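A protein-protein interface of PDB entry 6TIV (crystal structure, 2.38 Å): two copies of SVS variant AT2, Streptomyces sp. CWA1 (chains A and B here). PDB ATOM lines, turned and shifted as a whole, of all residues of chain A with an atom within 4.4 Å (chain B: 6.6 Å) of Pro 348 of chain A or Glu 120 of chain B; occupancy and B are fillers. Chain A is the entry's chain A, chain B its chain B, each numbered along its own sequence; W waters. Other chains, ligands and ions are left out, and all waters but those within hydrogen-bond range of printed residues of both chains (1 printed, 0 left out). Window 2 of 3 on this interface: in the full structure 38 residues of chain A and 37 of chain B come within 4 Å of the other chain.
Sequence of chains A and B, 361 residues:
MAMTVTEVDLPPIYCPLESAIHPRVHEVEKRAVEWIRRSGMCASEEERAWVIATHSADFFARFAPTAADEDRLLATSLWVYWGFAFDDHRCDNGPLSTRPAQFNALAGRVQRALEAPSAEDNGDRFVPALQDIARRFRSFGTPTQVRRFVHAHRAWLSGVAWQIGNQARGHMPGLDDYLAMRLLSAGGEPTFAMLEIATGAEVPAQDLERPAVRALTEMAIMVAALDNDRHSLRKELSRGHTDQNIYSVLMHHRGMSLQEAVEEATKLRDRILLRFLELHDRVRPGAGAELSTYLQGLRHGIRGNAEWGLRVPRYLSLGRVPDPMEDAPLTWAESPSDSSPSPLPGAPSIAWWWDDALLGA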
ATOM      1  N   ASP A 176      12.478  -3.152  20.504  1.00  0.00           N
ATOM      2  CA  ASP A 176      11.226  -2.374  20.688  1.00  0.00           C
ATOM      3  C   ASP A 176      10.072  -3.310  21.079  1.00  0.00           C
ATOM      4  O   ASP A 176       9.419  -3.057  22.114  1.00  0.00           O
ATOM      5  CB  ASP A 176      10.883  -1.550  19.452  1.00  0.00           C
ATOM      6  CG  ASP A 176       9.838  -0.486  19.763  1.00  0.00           C
ATOM      7  OD1 ASP A 176      10.004   0.253  20.753  1.00  0.00           O
ATOM      8  OD2 ASP A 176       8.853  -0.431  19.052  1.00  0.00           O
ATOM      9  N   GLY A 346      16.538   2.639  19.618  1.00  0.00           N
ATOM     10  CA  GLY A 346      15.891   1.482  18.981  1.00  0.00           C
ATOM     11  C   GLY A 346      14.621   1.061  19.690  1.00  0.00           C
ATOM     12  O   GLY A 346      14.069   0.051  19.242  1.00  0.00           O
ATOM     13  N   ALA A 347      14.157   1.819  20.704  1.00  0.00           N
ATOM     14  CA  ALA A 347      12.933   1.543  21.496  1.00  0.00           C
ATOM     15  C   ALA A 347      11.960   2.732  21.477  1.00  0.00           C
ATOM     16  O   ALA A 347      11.684   3.325  22.523  1.00  0.00           O
ATOM     17  CB  ALA A 347      13.338   1.185  22.897  1.00  0.00           C
ATOM     18  N   PRO A 348      11.446   3.136  20.279  1.00  0.00           N
ATOM     19  CA  PRO A 348      10.502   4.260  20.144  1.00  0.00           C
ATOM     20  C   PRO A 348       9.266   4.139  21.057  1.00  0.00           C
ATOM     21  O   PRO A 348       8.806   5.123  21.678  1.00  0.00           O
ATOM     22  CB  PRO A 348      10.147   4.224  18.659  1.00  0.00           C
ATOM     23  CG  PRO A 348      10.588   2.853  18.174  1.00  0.00           C
ATOM     24  CD  PRO A 348      11.826   2.567  18.968  1.00  0.00           C
ATOM     25  N   SER A 349       8.796   2.920  21.254  1.00  0.00           N
ATOM     26  CA  SER A 349       7.534   2.688  22.002  1.00  0.00           C
ATOM     27  C   SER A 349       7.687   3.070  23.477  1.00  0.00           C
ATOM     28  O   SER A 349       6.655   3.186  24.109  1.00  0.00           O
ATOM     29  CB  SER A 349       6.988   1.276  21.805  1.00  0.00           C
ATOM     30  OG  SER A 349       6.968   0.581  23.039  1.00  0.00           O
ATOM     31  N   ILE A 350       8.901   3.305  23.998  1.00  0.00           N
ATOM     32  CA  ILE A 350       9.101   3.825  25.380  1.00  0.00           C
ATOM     33  C   ILE A 350       9.640   5.258  25.396  1.00  0.00           C
ATOM     34  O   ILE A 350       9.756   5.787  26.502  1.00  0.00           O
ATOM     35  CB  ILE A 350       9.991   2.888  26.192  1.00  0.00           C
ATOM     36  CG1 ILE A 350      11.400   2.830  25.612  1.00  0.00           C
ATOM     37  CG2 ILE A 350       9.335   1.500  26.351  1.00  0.00           C
ATOM     38  CD1 ILE A 350      12.435   2.389  26.620  1.00  0.00           C
ATOM     39  N   ALA A 351       9.931   5.879  24.256  1.00  0.00           N
ATOM     40  CA  ALA A 351      10.564   7.221  24.178  1.00  0.00           C
ATOM     41  C   ALA A 351       9.696   8.259  24.900  1.00  0.00           C
ATOM     42  O   ALA A 351      10.242   9.184  25.479  1.00  0.00           O
ATOM     43  CB  ALA A 351      10.815   7.619  22.739  1.00  0.00           C
ATOM     44  N   ALA B 113       0.581   0.963  20.586  1.00  0.00           N
ATOM     45  CA  ALA B 113       0.586   2.216  19.795  1.00  0.00           C
ATOM     46  C   ALA B 113      -0.504   3.147  20.326  1.00  0.00           C
ATOM     47  O   ALA B 113      -0.334   4.382  20.212  1.00  0.00           O
ATOM     48  CB  ALA B 113       0.424   1.945  18.319  1.00  0.00           C
ATOM     49  N   ALA B 116       1.114   4.439  23.761  1.00  0.00           N
ATOM     50  CA  ALA B 116       2.476   5.000  23.580  1.00  0.00           C
ATOM     51  C   ALA B 116       2.522   5.868  22.327  1.00  0.00           C
ATOM     52  O   ALA B 116       2.762   5.359  21.242  1.00  0.00           O
ATOM     53  CB  ALA B 116       3.428   3.846  23.466  1.00  0.00           C
ATOM     54  N   PRO B 117       2.310   7.201  22.409  1.00  0.00           N
ATOM     55  CA  PRO B 117       2.328   8.059  21.225  1.00  0.00           C
ATOM     56  C   PRO B 117       3.641   8.000  20.451  1.00  0.00           C
ATOM     57  O   PRO B 117       3.630   8.331  19.302  1.00  0.00           O
ATOM     58  CB  PRO B 117       2.122   9.480  21.774  1.00  0.00           C
ATOM     59  CG  PRO B 117       1.410   9.247  23.063  1.00  0.00           C
ATOM     60  CD  PRO B 117       2.027   7.980  23.630  1.00  0.00           C
ATOM     61  N   SER B 118       4.727   7.604  21.094  1.00  0.00           N
ATOM     62  CA  SER B 118       6.075   7.546  20.477  1.00  0.00           C
ATOM     63  C   SER B 118       6.260   6.236  19.679  1.00  0.00           C
ATOM     64  O   SER B 118       7.246   6.143  18.949  1.00  0.00           O
ATOM     65  CB  SER B 118       7.113   7.698  21.536  1.00  0.00           C
ATOM     66  OG  SER B 118       6.951   6.673  22.517  1.00  0.00           O
ATOM     67  N   ALA B 119       5.370   5.245  19.811  1.00  0.00           N
ATOM     68  CA  ALA B 119       5.497   3.957  19.088  1.00  0.00           C
ATOM     69  C   ALA B 119       5.579   4.251  17.590  1.00  0.00           C
ATOM     70  O   ALA B 119       4.971   5.213  17.207  1.00  0.00           O
ATOM     71  CB  ALA B 119       4.325   3.053  19.408  1.00  0.00           C
ATOM     72  N   GLU B 120       6.252   3.449  16.769  1.00  0.00           N
ATOM     73  CA  GLU B 120       6.394   3.764  15.310  1.00  0.00           C
ATOM     74  C   GLU B 120       5.629   2.717  14.491  1.00  0.00           C
ATOM     75  O   GLU B 120       5.505   1.617  14.939  1.00  0.00           O
ATOM     76  CB  GLU B 120       7.866   4.001  14.933  1.00  0.00           C
ATOM     77  CG  GLU B 120       8.377   5.252  15.654  1.00  0.00           C
ATOM     78  CD  GLU B 120       9.741   5.848  15.321  1.00  0.00           C
ATOM     79  OE1 GLU B 120      10.454   5.263  14.428  1.00  0.00           O
ATOM     80  OE2 GLU B 120      10.095   6.906  15.980  1.00  0.00           O
ATOM     81  N   ASP B 121       5.084   3.108  13.341  1.00  0.00           N
ATOM     82  CA  ASP B 121       4.136   2.286  12.540  1.00  0.00           C
ATOM     83  C   ASP B 121       4.817   0.995  12.069  1.00  0.00           C
ATOM     84  O   ASP B 121       4.252  -0.090  12.313  1.00  0.00           O
ATOM     85  CB  ASP B 121       3.530   3.116  11.412  1.00  0.00           C
ATOM     86  CG  ASP B 121       4.506   3.535  10.332  1.00  0.00           C
ATOM     87  OD1 ASP B 121       4.833   4.762  10.274  1.00  0.00           O
ATOM     88  OD2 ASP B 121       4.897   2.643   9.546  1.00  0.00           O
ATOM     89  N   ASN B 122       5.998   1.093  11.450  1.00  0.00           N
ATOM     90  CA  ASN B 122       6.742  -0.089  10.934  1.00  0.00           C
ATOM     91  C   ASN B 122       5.957  -0.661   9.742  1.00  0.00           C
ATOM     92  O   ASN B 122       5.840  -1.925   9.629  1.00  0.00           O
ATOM     93  CB  ASN B 122       7.013  -1.100  12.059  1.00  0.00           C
ATOM     94  CG  ASN B 122       8.475  -1.150  12.460  1.00  0.00           C
ATOM     95  OD1 ASN B 122       9.115  -2.186  12.294  1.00  0.00           O
ATOM     96  ND2 ASN B 122       9.012  -0.043  12.960  1.00  0.00           N
ATOM     97  N   GLY B 123       5.409   0.259   8.929  1.00  0.00           N
ATOM     98  CA  GLY B 123       4.614   0.014   7.710  1.00  0.00           C
ATOM     99  C   GLY B 123       3.302  -0.723   7.955  1.00  0.00           C
ATOM    100  O   GLY B 123       2.660  -1.093   6.966  1.00  0.00           O
ATOM    101  N   VAL B 127      -1.755   1.393  12.345  1.00  0.00           N
ATOM    102  CA  VAL B 127      -1.171   1.979  13.589  1.00  0.00           C
ATOM    103  C   VAL B 127      -1.204   3.514  13.542  1.00  0.00           C
ATOM    104  O   VAL B 127      -1.667   4.145  14.493  1.00  0.00           O
ATOM    105  CB  VAL B 127       0.223   1.396  13.879  1.00  0.00           C
ATOM    106  CG1 VAL B 127       1.032   2.292  14.804  1.00  0.00           C
ATOM    107  CG2 VAL B 127       0.118  -0.020  14.427  1.00  0.00           C
ATOM    108  N   GLN B 131      -3.339   5.910  16.035  1.00  0.00           N
ATOM    109  CA  GLN B 131      -2.537   6.903  16.794  1.00  0.00           C
ATOM    110  C   GLN B 131      -3.116   8.304  16.553  1.00  0.00           C
ATOM    111  O   GLN B 131      -3.104   9.109  17.531  1.00  0.00           O
ATOM    112  CB  GLN B 131      -1.056   6.738  16.430  1.00  0.00           C
ATOM    113  CG  GLN B 131      -0.317   5.734  17.313  1.00  0.00           C
ATOM    114  CD  GLN B 131       1.156   5.758  17.001  1.00  0.00           C
ATOM    115  OE1 GLN B 131       1.539   6.042  15.878  1.00  0.00           O
ATOM    116  NE2 GLN B 131       1.996   5.474  17.982  1.00  0.00           N
HETATM  117  O   HOH W   1       7.135   1.097  18.310  1.00  0.00           O
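OG of Ser 118 of chain B lies within hydrogen-bond range of O of Pro 348 of chain A (2.6 Å).
O of Ala 119 of chain B is in hydrogen-bond range of NE2 of Gln 131 of chain B.
The backbone carbonyl oxygen (O) of Ala 116 of chain B lies within hydrogen-bond range of the side-chain amide nitrogen (NE2) of Gln 131 of chain B (3.4 Å).
The side-chain carboxylate of Asp 176 of chain A lies within hydrogen-bond range of the backbone NH of Ser 349 of chain A (3.0 Å).
O of Pro 348 of chain A touches N of Ala 119 of chain B, at 3.9 Å.
Glu 120 of chain B touches Pro 348 of chain A.
O of Ser 349 of chain A touches CB of Ala 116 of chain B, 3.4 Å away.
Ser 349 of chain A touches Ser 118 of chain B (C to OG, 3.8 Å).
Ser 349 of chain A touches Ala 119 of chain B.
Ser 118 of chain B touches Ala 351 of chain A.
Pro 348 of chain A touches just these residues of chain B: Ser 118, Ala 119 and Glu 120.
Glu 120 of chain B touches just one residue of chain A: Pro 348.
Printed residues of chain A within 4 Å of Ala 119 of chain B: Pro 348 (3.9 Å) and Ser 349 (3.8 Å).
Printed residues of chain B within 4 Å of Ser 349 of chain A: Ala 116 (3.4 Å), Ser 118 (3.8 Å) and Ala 119 (3.8 Å).
Gly 346 of chain A touches none of the printed residues of chain B.
The nearest residue of chain B that does not touch Pro 348 of chain A is Ala 116 of chain B (5.8 Å).
The nearest printed residue of chain A that does not touch Glu 120 of chain B is Ser 349 of chain A (5.2 Å).
The nearest printed residue of chain B that does not touch Ala 351 of chain A is Ala 119 of chain B (6.4 Å).
Of the 11 printed residues of chain B, 4 touch a printed residue of chain A.
Hydrophobic or aromatic side chains of chain B that line the printed part of chain A: Ala 116 and Ala 119.
Among the printed residues, no Asp or Glu carboxylate lies within 4 Å of a Lys or Arg side-chain nitrogen of the other chain.
No position is printed for both chains.
Of the 7 pairs that touch across the chains among the printed residues, none has its exchanged pair printed and touching as well.
Water W1 lies within hydrogen-bond range of the side-chain carboxylate (OD2) of Asp 176 of chain A (2.4 Å) and the backbone NH (N) of Glu 120 of chain B (2.9 Å).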
